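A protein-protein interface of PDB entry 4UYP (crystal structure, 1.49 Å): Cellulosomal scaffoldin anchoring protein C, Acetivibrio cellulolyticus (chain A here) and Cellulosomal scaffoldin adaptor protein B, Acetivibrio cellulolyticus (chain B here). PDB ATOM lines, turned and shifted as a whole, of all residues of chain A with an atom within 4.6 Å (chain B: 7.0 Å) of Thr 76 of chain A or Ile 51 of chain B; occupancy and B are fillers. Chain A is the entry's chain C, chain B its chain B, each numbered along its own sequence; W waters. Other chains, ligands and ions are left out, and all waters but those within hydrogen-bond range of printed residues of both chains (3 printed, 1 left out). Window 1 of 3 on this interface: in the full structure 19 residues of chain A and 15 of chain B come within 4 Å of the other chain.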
ATOM      1  N   ALA A  33       1.243 -23.458  -1.392  1.00  0.00           N
ATOM      2  CA  ALA A  33       0.072 -23.594  -2.307  1.00  0.00           C
ATOM      3  C   ALA A  33       0.575 -23.155  -3.668  1.00  0.00           C
ATOM      4  O   ALA A  33       1.392 -22.273  -3.810  1.00  0.00           O
ATOM      5  CB  ALA A  33      -1.108 -22.717  -1.873  1.00  0.00           C
ATOM      6  N   LEU A  34       0.029 -23.764  -4.725  1.00  0.00           N
ATOM      7  CA  LEU A  34       0.383 -23.362  -6.104  1.00  0.00           C
ATOM      8  C   LEU A  34      -0.721 -23.830  -6.999  1.00  0.00           C
ATOM      9  O   LEU A  34      -1.466 -24.793  -6.747  1.00  0.00           O
ATOM     10  CB  LEU A  34       1.742 -23.976  -6.535  1.00  0.00           C
ATOM     11  CG  LEU A  34       1.716 -25.491  -6.844  1.00  0.00           C
ATOM     12  CD1 LEU A  34       1.590 -25.661  -8.386  1.00  0.00           C
ATOM     13  CD2 LEU A  34       3.049 -26.100  -6.339  1.00  0.00           C
ATOM     14  N   SER A  35      -0.854 -23.100  -8.106  1.00  0.00           N
ATOM     15  CA  SER A  35      -1.603 -23.642  -9.287  1.00  0.00           C
ATOM     16  C   SER A  35      -0.659 -23.571 -10.491  1.00  0.00           C
ATOM     17  O   SER A  35       0.206 -22.732 -10.572  1.00  0.00           O
ATOM     18  CB  SER A  35      -2.882 -22.847  -9.551  1.00  0.00           C
ATOM     19  OG  SER A  35      -2.565 -21.518  -9.921  1.00  0.00           O
ATOM     20  N   ASP A  61      -3.640 -33.530  -1.093  1.00  0.00           N
ATOM     21  CA  ASP A  61      -3.117 -32.164  -1.281  1.00  0.00           C
ATOM     22  C   ASP A  61      -3.126 -31.742  -2.749  1.00  0.00           C
ATOM     23  O   ASP A  61      -2.840 -30.560  -3.083  1.00  0.00           O
ATOM     24  CB  ASP A  61      -1.669 -32.081  -0.761  1.00  0.00           C
ATOM     25  CG  ASP A  61      -1.533 -32.568   0.693  1.00  0.00           C
ATOM     26  OD1 ASP A  61      -2.516 -32.476   1.419  1.00  0.00           O
ATOM     27  OD2 ASP A  61      -0.413 -32.951   1.006  1.00  0.00           O
ATOM     28  N   PHE A  62      -3.398 -32.643  -3.672  1.00  0.00           N
ATOM     29  CA  PHE A  62      -3.188 -32.436  -5.124  1.00  0.00           C
ATOM     30  C   PHE A  62      -4.465 -32.682  -5.902  1.00  0.00           C
ATOM     31  O   PHE A  62      -5.173 -33.616  -5.686  1.00  0.00           O
ATOM     32  CB  PHE A  62      -2.146 -33.493  -5.570  1.00  0.00           C
ATOM     33  CG  PHE A  62      -1.763 -33.429  -7.039  1.00  0.00           C
ATOM     34  CD1 PHE A  62      -0.896 -32.423  -7.511  1.00  0.00           C
ATOM     35  CD2 PHE A  62      -2.186 -34.446  -7.890  1.00  0.00           C
ATOM     36  CE1 PHE A  62      -0.504 -32.420  -8.814  1.00  0.00           C
ATOM     37  CE2 PHE A  62      -1.781 -34.442  -9.197  1.00  0.00           C
ATOM     38  CZ  PHE A  62      -0.943 -33.448  -9.685  1.00  0.00           C
ATOM     39  N   THR A  63      -4.811 -31.696  -6.729  1.00  0.00           N
ATOM     40  CA  THR A  63      -6.050 -31.724  -7.498  1.00  0.00           C
ATOM     41  C   THR A  63      -5.737 -31.418  -8.940  1.00  0.00           C
ATOM     42  O   THR A  63      -4.889 -30.532  -9.236  1.00  0.00           O
ATOM     43  CB  THR A  63      -7.070 -30.662  -7.033  1.00  0.00           C
ATOM     44  OG1 THR A  63      -7.163 -30.812  -5.591  1.00  0.00           O
ATOM     45  CG2 THR A  63      -8.428 -30.966  -7.622  1.00  0.00           C
ATOM     46  N   SER A  74      -4.848 -28.188 -15.700  1.00  0.00           N
ATOM     47  CA  SER A  74      -4.569 -27.407 -14.453  1.00  0.00           C
ATOM     48  C   SER A  74      -4.301 -28.361 -13.319  1.00  0.00           C
ATOM     49  O   SER A  74      -4.943 -29.398 -13.210  1.00  0.00           O
ATOM     50  CB  SER A  74      -5.743 -26.546 -14.000  1.00  0.00           C
ATOM     51  OG  SER A  74      -6.130 -25.629 -15.050  1.00  0.00           O
ATOM     52  N   MET A  75      -3.370 -27.972 -12.494  1.00  0.00           N
ATOM     53  CA  MET A  75      -2.936 -28.757 -11.307  1.00  0.00           C
ATOM     54  C   MET A  75      -2.900 -27.788 -10.114  1.00  0.00           C
ATOM     55  O   MET A  75      -2.359 -26.686 -10.278  1.00  0.00           O
ATOM     56  CB  MET A  75      -1.527 -29.374 -11.584  1.00  0.00           C
ATOM     57  CG  MET A  75      -1.627 -30.621 -12.513  1.00  0.00           C
ATOM     58  SD  MET A  75      -0.409 -30.503 -13.869  1.00  0.00           S
ATOM     59  CE  MET A  75      -1.100 -29.243 -14.991  1.00  0.00           C
ATOM     60  N   THR A  76      -3.361 -28.240  -8.961  1.00  0.00           N
ATOM     61  CA  THR A  76      -3.121 -27.436  -7.723  1.00  0.00           C
ATOM     62  C   THR A  76      -2.504 -28.290  -6.659  1.00  0.00           C
ATOM     63  O   THR A  76      -2.736 -29.502  -6.554  1.00  0.00           O
ATOM     64  CB  THR A  76      -4.382 -26.799  -7.105  1.00  0.00           C
ATOM     65  OG1 THR A  76      -5.394 -27.794  -6.808  1.00  0.00           O
ATOM     66  CG2 THR A  76      -4.989 -25.821  -8.140  1.00  0.00           C
ATOM     67  N   PHE A  77      -1.687 -27.621  -5.832  1.00  0.00           N
ATOM     68  CA  PHE A  77      -1.167 -28.201  -4.572  1.00  0.00           C
ATOM     69  C   PHE A  77      -1.543 -27.283  -3.439  1.00  0.00           C
ATOM     70  O   PHE A  77      -1.425 -26.041  -3.544  1.00  0.00           O
ATOM     71  CB  PHE A  77       0.352 -28.290  -4.628  1.00  0.00           C
ATOM     72  CG  PHE A  77       0.982 -28.744  -3.329  1.00  0.00           C
ATOM     73  CD1 PHE A  77       0.876 -30.071  -2.895  1.00  0.00           C
ATOM     74  CD2 PHE A  77       1.633 -27.832  -2.522  1.00  0.00           C
ATOM     75  CE1 PHE A  77       1.451 -30.501  -1.705  1.00  0.00           C
ATOM     76  CE2 PHE A  77       2.204 -28.244  -1.312  1.00  0.00           C
ATOM     77  CZ  PHE A  77       2.115 -29.556  -0.904  1.00  0.00           C
ATOM     78  N   GLU A  78      -2.114 -27.870  -2.375  1.00  0.00           N
ATOM     79  CA  GLU A  78      -2.435 -27.119  -1.141  1.00  0.00           C
ATOM     80  C   GLU A  78      -1.849 -27.938   0.001  1.00  0.00           C
ATOM     81  O   GLU A  78      -2.412 -29.042   0.286  1.00  0.00           O
ATOM     82  CB  GLU A  78      -3.908 -26.953  -1.007  1.00  0.00           C
ATOM     83  CG  GLU A  78      -4.618 -26.165  -2.161  1.00  0.00           C
ATOM     84  CD  GLU A  78      -6.121 -26.573  -2.306  1.00  0.00           C
ATOM     85  OE1 GLU A  78      -6.424 -27.789  -2.506  1.00  0.00           O
ATOM     86  OE2 GLU A  78      -6.876 -25.556  -2.186  1.00  0.00           O
ATOM     87  N   SER A 120       0.519 -19.782 -10.250  1.00  0.00           N
ATOM     88  CA  SER A 120       1.091 -18.914  -9.166  1.00  0.00           C
ATOM     89  C   SER A 120       1.582 -19.846  -8.090  1.00  0.00           C
ATOM     90  O   SER A 120       1.110 -20.974  -7.919  1.00  0.00           O
ATOM     91  CB  SER A 120       0.081 -17.965  -8.509  1.00  0.00           C
ATOM     92  OG  SER A 120      -0.939 -18.606  -7.734  1.00  0.00           O
ATOM     93  N   TYR A 122       3.008 -19.961  -3.852  1.00  0.00           N
ATOM     94  CA  TYR A 122       2.926 -19.217  -2.531  1.00  0.00           C
ATOM     95  C   TYR A 122       3.778 -19.919  -1.483  1.00  0.00           C
ATOM     96  O   TYR A 122       3.696 -21.121  -1.288  1.00  0.00           O
ATOM     97  CB  TYR A 122       1.510 -19.141  -2.066  1.00  0.00           C
ATOM     98  CG  TYR A 122       0.701 -18.080  -2.815  1.00  0.00           C
ATOM     99  CD1 TYR A 122       0.162 -18.325  -4.107  1.00  0.00           C
ATOM    100  CD2 TYR A 122       0.571 -16.797  -2.290  1.00  0.00           C
ATOM    101  CE1 TYR A 122      -0.478 -17.314  -4.775  1.00  0.00           C
ATOM    102  CE2 TYR A 122      -0.043 -15.795  -3.004  1.00  0.00           C
ATOM    103  CZ  TYR A 122      -0.587 -16.055  -4.226  1.00  0.00           C
ATOM    104  OH  TYR A 122      -1.213 -15.056  -4.986  1.00  0.00           O
ATOM    105  N   ALA B  18     -14.045 -23.260  -0.085  1.00  0.00           N
ATOM    106  CA  ALA B  18     -12.660 -23.221  -0.564  1.00  0.00           C
ATOM    107  C   ALA B  18     -12.536 -24.178  -1.746  1.00  0.00           C
ATOM    108  O   ALA B  18     -11.701 -23.942  -2.619  1.00  0.00           O
ATOM    109  CB  ALA B  18     -11.714 -23.683   0.594  1.00  0.00           C
ATOM    110  N   ILE B  21     -13.561 -22.207  -4.817  1.00  0.00           N
ATOM    111  CA  ILE B  21     -12.542 -21.320  -5.312  1.00  0.00           C
ATOM    112  C   ILE B  21     -11.485 -22.154  -6.069  1.00  0.00           C
ATOM    113  O   ILE B  21     -11.022 -21.704  -7.154  1.00  0.00           O
ATOM    114  CB  ILE B  21     -11.867 -20.575  -4.157  1.00  0.00           C
ATOM    115  CG1 ILE B  21     -12.909 -19.670  -3.458  1.00  0.00           C
ATOM    116  CG2 ILE B  21     -10.765 -19.700  -4.682  1.00  0.00           C
ATOM    117  CD1 ILE B  21     -12.357 -18.953  -2.200  1.00  0.00           C
ATOM    118  N   ARG B  22     -11.090 -23.304  -5.510  1.00  0.00           N
ATOM    119  CA  ARG B  22     -10.152 -24.174  -6.252  1.00  0.00           C
ATOM    120  C   ARG B  22     -10.743 -24.594  -7.661  1.00  0.00           C
ATOM    121  O   ARG B  22      -9.977 -24.588  -8.669  1.00  0.00           O
ATOM    122  CB  ARG B  22      -9.802 -25.357  -5.360  1.00  0.00           C
ATOM    123  CG  ARG B  22      -8.782 -26.302  -6.052  1.00  0.00           C
ATOM    124  CD  ARG B  22      -8.429 -27.413  -5.075  1.00  0.00           C
ATOM    125  NE  ARG B  22      -9.572 -28.321  -4.892  1.00  0.00           N
ATOM    126  CZ  ARG B  22      -9.683 -29.143  -3.858  1.00  0.00           C
ATOM    127  NH1 ARG B  22      -8.850 -29.137  -2.830  1.00  0.00           N
ATOM    128  NH2 ARG B  22     -10.689 -30.003  -3.896  1.00  0.00           N
ATOM    129  N   VAL B  25     -10.002 -21.696  -9.981  1.00  0.00           N
ATOM    130  CA  VAL B  25      -8.619 -21.661 -10.359  1.00  0.00           C
ATOM    131  C   VAL B  25      -8.250 -22.769 -11.372  1.00  0.00           C
ATOM    132  O   VAL B  25      -7.463 -22.522 -12.321  1.00  0.00           O
ATOM    133  CB  VAL B  25      -7.770 -21.708  -9.065  1.00  0.00           C
ATOM    134  CG1 VAL B  25      -6.299 -21.756  -9.483  1.00  0.00           C
ATOM    135  CG2 VAL B  25      -8.015 -20.474  -8.204  1.00  0.00           C
ATOM    136  N   LEU B  26      -8.804 -23.948 -11.145  1.00  0.00           N
ATOM    137  CA  LEU B  26      -8.592 -25.115 -12.048  1.00  0.00           C
ATOM    138  C   LEU B  26      -9.221 -24.911 -13.410  1.00  0.00           C
ATOM    139  O   LEU B  26      -8.863 -25.621 -14.375  1.00  0.00           O
ATOM    140  CB  LEU B  26      -9.126 -26.367 -11.403  1.00  0.00           C
ATOM    141  CG  LEU B  26      -8.323 -27.006 -10.222  1.00  0.00           C
ATOM    142  CD1 LEU B  26      -9.168 -28.021  -9.480  1.00  0.00           C
ATOM    143  CD2 LEU B  26      -7.011 -27.583 -10.718  1.00  0.00           C
ATOM    144  N   ILE B  49      -8.859 -13.751  -8.310  1.00  0.00           N
ATOM    145  CA  ILE B  49      -9.055 -15.029  -7.626  1.00  0.00           C
ATOM    146  C   ILE B  49      -7.849 -15.939  -7.960  1.00  0.00           C
ATOM    147  O   ILE B  49      -7.575 -16.200  -9.149  1.00  0.00           O
ATOM    148  CB  ILE B  49     -10.374 -15.621  -8.038  1.00  0.00           C
ATOM    149  CG1 ILE B  49     -11.500 -14.563  -7.907  1.00  0.00           C
ATOM    150  CG2 ILE B  49     -10.748 -16.832  -7.188  1.00  0.00           C
ATOM    151  CD1 ILE B  49     -12.895 -15.137  -8.138  1.00  0.00           C
ATOM    152  N   LYS B  50      -7.126 -16.366  -6.947  1.00  0.00           N
ATOM    153  CA  LYS B  50      -5.936 -17.199  -7.113  1.00  0.00           C
ATOM    154  C   LYS B  50      -5.949 -18.258  -6.102  1.00  0.00           C
ATOM    155  O   LYS B  50      -6.775 -18.335  -5.194  1.00  0.00           O
ATOM    156  CB  LYS B  50      -4.681 -16.386  -6.996  1.00  0.00           C
ATOM    157  CG  LYS B  50      -4.588 -15.175  -7.980  1.00  0.00           C
ATOM    158  CD  LYS B  50      -3.354 -14.348  -7.759  1.00  0.00           C
ATOM    159  CE  LYS B  50      -2.126 -15.058  -8.183  1.00  0.00           C
ATOM    160  NZ  LYS B  50      -0.900 -14.187  -8.070  1.00  0.00           N
ATOM    161  N   ILE B  51      -5.003 -19.241  -6.244  1.00  0.00           N
ATOM    162  CA  ILE B  51      -5.037 -20.369  -5.345  1.00  0.00           C
ATOM    163  C   ILE B  51      -4.917 -19.977  -3.860  1.00  0.00           C
ATOM    164  O   ILE B  51      -5.431 -20.729  -3.015  1.00  0.00           O
ATOM    165  CB  ILE B  51      -3.941 -21.461  -5.780  1.00  0.00           C
ATOM    166  CG1 ILE B  51      -4.155 -22.849  -5.074  1.00  0.00           C
ATOM    167  CG2 ILE B  51      -2.542 -20.948  -5.528  1.00  0.00           C
ATOM    168  CD1 ILE B  51      -5.532 -23.432  -5.301  1.00  0.00           C
ATOM    169  N   ASN B  52      -4.184 -18.895  -3.583  1.00  0.00           N
ATOM    170  CA  ASN B  52      -4.080 -18.631  -2.145  1.00  0.00           C
ATOM    171  C   ASN B  52      -5.394 -18.148  -1.567  1.00  0.00           C
ATOM    172  O   ASN B  52      -5.586 -18.367  -0.361  1.00  0.00           O
ATOM    173  CB  ASN B  52      -3.016 -17.548  -1.928  1.00  0.00           C
ATOM    174  CG  ASN B  52      -3.451 -16.186  -2.422  1.00  0.00           C
ATOM    175  OD1 ASN B  52      -3.928 -16.008  -3.557  1.00  0.00           O
ATOM    176  ND2 ASN B  52      -3.302 -15.147  -1.557  1.00  0.00           N
ATOM    177  N   ASP B  53      -6.320 -17.608  -2.347  1.00  0.00           N
ATOM    178  CA  ASP B  53      -7.665 -17.296  -1.802  1.00  0.00           C
ATOM    179  C   ASP B  53      -8.301 -18.556  -1.333  1.00  0.00           C
ATOM    180  O   ASP B  53      -8.964 -18.593  -0.299  1.00  0.00           O
ATOM    181  CB  ASP B  53      -8.519 -16.603  -2.841  1.00  0.00           C
ATOM    182  CG  ASP B  53      -7.996 -15.264  -3.262  1.00  0.00           C
ATOM    183  OD1 ASP B  53      -7.857 -14.316  -2.434  1.00  0.00           O
ATOM    184  OD2 ASP B  53      -7.757 -15.004  -4.498  1.00  0.00           O
ATOM    185  N   ALA B  54      -8.125 -19.696  -2.095  1.00  0.00           N
ATOM    186  CA  ALA B  54      -8.791 -20.920  -1.692  1.00  0.00           C
ATOM    187  C   ALA B  54      -8.167 -21.432  -0.362  1.00  0.00           C
ATOM    188  O   ALA B  54      -8.925 -21.872   0.501  1.00  0.00           O
ATOM    189  CB  ALA B  54      -8.561 -21.975  -2.857  1.00  0.00           C
ATOM    190  N   VAL B  55      -6.855 -21.382  -0.240  1.00  0.00           N
ATOM    191  CA  VAL B  55      -6.243 -21.906   0.957  1.00  0.00           C
ATOM    192  C   VAL B  55      -6.530 -21.002   2.163  1.00  0.00           C
ATOM    193  O   VAL B  55      -6.703 -21.546   3.263  1.00  0.00           O
ATOM    194  CB  VAL B  55      -4.773 -22.243   0.762  1.00  0.00           C
ATOM    195  CG1 VAL B  55      -3.831 -21.022   0.860  1.00  0.00           C
ATOM    196  CG2 VAL B  55      -4.391 -23.448   1.592  1.00  0.00           C
ATOM    197  N   LEU B  56      -6.684 -19.694   1.905  1.00  0.00           N
ATOM    198  CA  LEU B  56      -7.123 -18.802   2.999  1.00  0.00           C
ATOM    199  C   LEU B  56      -8.484 -19.163   3.478  1.00  0.00           C
ATOM    200  O   LEU B  56      -8.722 -19.177   4.722  1.00  0.00           O
ATOM    201  CB  LEU B  56      -7.015 -17.343   2.559  1.00  0.00           C
ATOM    202  CG  LEU B  56      -5.586 -16.756   2.459  1.00  0.00           C
ATOM    203  CD1 LEU B  56      -5.586 -15.425   1.716  1.00  0.00           C
ATOM    204  CD2 LEU B  56      -4.931 -16.548   3.875  1.00  0.00           C
HETATM  205  O   HOH W   1      -4.793 -23.188 -12.998  1.00  0.00           O
HETATM  206  O   HOH W   2      -9.458 -25.862  -1.779  1.00  0.00           O
HETATM  207  O   HOH W   3      -3.394 -19.198  -8.671  1.00  0.00           O
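The side-chain hydroxyl (OG) of Ser 74 of chain A sits at hydrogen-bond distance from the backbone carbonyl oxygen (O) of Leu 26 of chain B.
The guanidinium group (NH1) of Arg 22 of chain B is in salt-bridge range of the side-chain carboxylate (OE1) of Glu 78 of chain A (2.8 Å).
NZ of Lys 50 of chain B is in hydrogen-bond range of OH of Tyr 122 of chain A, 3.2 Å away.
The side-chain hydroxyl of Tyr 122 of chain A is in hydrogen-bond range of the side-chain amide oxygen of Asn 52 of chain B (3.2 Å).
The backbone NH (N) of Tyr 122 of chain A sits at hydrogen-bond distance from the backbone carbonyl oxygen (O) of Ala 33 of chain A (2.8 Å).
N of Leu 34 of chain A is in hydrogen-bond range of O of Phe 77 of chain A (2.9 Å).
N of Ser 35 of chain A sits at hydrogen-bond distance from O of Ser 120 of chain A (2.9 Å).
O of Asp 61 of chain A is in hydrogen-bond range of N of Glu 78 of chain A.
The backbone carbonyl oxygen (O) of Thr 63 of chain A is in hydrogen-bond range of the backbone NH (N) of Thr 76 of chain A (2.8 Å).
The backbone NH of Lys 50 of chain B sits close to the side-chain carboxylate of Asp 53 of chain B (2.9 Å).
Leu 34 of chain A touches Ile 51 of chain B (C to CG2, 3.7 Å).
Ser 35 of chain A touches Val 25 of chain B (CB to CG1, 3.6 Å).
N of Ser 35 of chain A touches CG2 of Ile 51 of chain B (3.8 Å).
OG1 of Thr 63 of chain A touches CZ of Arg 22 of chain B (3.5 Å).
Thr 63 of chain A touches Leu 26 of chain B.
Thr 76 of chain A touches Arg 22 of chain B (OG1 to CD, 3.5 Å).
CD2 of Leu 26 of chain B touches CG2 of Thr 76 of chain A, at 3.7 Å.
Thr 76 of chain A touches Ile 51 of chain B.
Lys 50 of chain B touches Ser 120 of chain A (CE to CB, 3.7 Å).
Ile 51 of chain B touches Ser 120 of chain A.
Of chain B, only Arg 22, Leu 26 and Ile 51 come within 4 Å of Thr 76 of chain A.
Of the printed residues of chain A, Ile 51 of chain B touches Leu 34 (3.7 Å), Ser 35 (3.8 Å), Thr 76 (3.7 Å) and Ser 120 (3.6 Å).
Printed residues of chain B within 4 Å of Tyr 122 of chain A: Lys 50 (3.2 Å) and Asn 52 (3.2 Å).
Of the printed residues of chain B, Ser 120 of chain A touches Lys 50 and Ile 51.
Of the printed residues of chain A, Leu 26 of chain B touches Thr 63, Ser 74 and Thr 76.
Of the printed residues of chain B, Ser 74 of chain A touches Leu 26.
Ala 54 of chain B touches none of the printed residues of chain A.
The nearest residue of chain B that does not touch Thr 76 of chain A is Val 25 of chain B (4.5 Å).
The nearest printed residue of chain A that does not touch Ile 51 of chain B is Glu 78 of chain A (4.003 Å).
The nearest printed residue of chain A that does not touch Leu 26 of chain B is Met 75 of chain A (4.1 Å).
Of the 13 printed residues of chain B, 6 touch a printed residue of chain A.
Along chain B the printed residues that touch a printed residue of chain A span positions 22 to 52.
Of the 13 printed residues of chain A, 8 touch a printed residue of chain B.
Printed residues of chain A that touch a printed residue of chain B: Leu 34, Ser 35, Thr 63, Ser 74, Thr 76, Glu 78, Ser 120 and Tyr 122.
Hydrophobic or aromatic side chains of chain A that line the printed part of chain B: Tyr 122.
Among the printed residues, 14 pairs touch across the chains.
Water W2 lies within hydrogen-bond range of the side-chain carboxylate (OE2) of Glu 78 of chain A (2.6 Å), the backbone carbonyl oxygen (O) of Ala 18 of chain B (3.1 Å) and the guanidinium group (NH1) of Arg 22 of chain B (3.5 Å).
Water W3 lies within hydrogen-bond range of the side-chain hydroxyl (OG) of Ser 120 of chain A, the side-chain hydroxyl (OG) of Ser 35 of chain A and the backbone NH (N) of Ile 51 of chain B.
Water W1 lies within hydrogen-bond range of O of Val 25 of chain B (2.8 Å) and OG of Ser 74 of chain A (3.5 Å).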
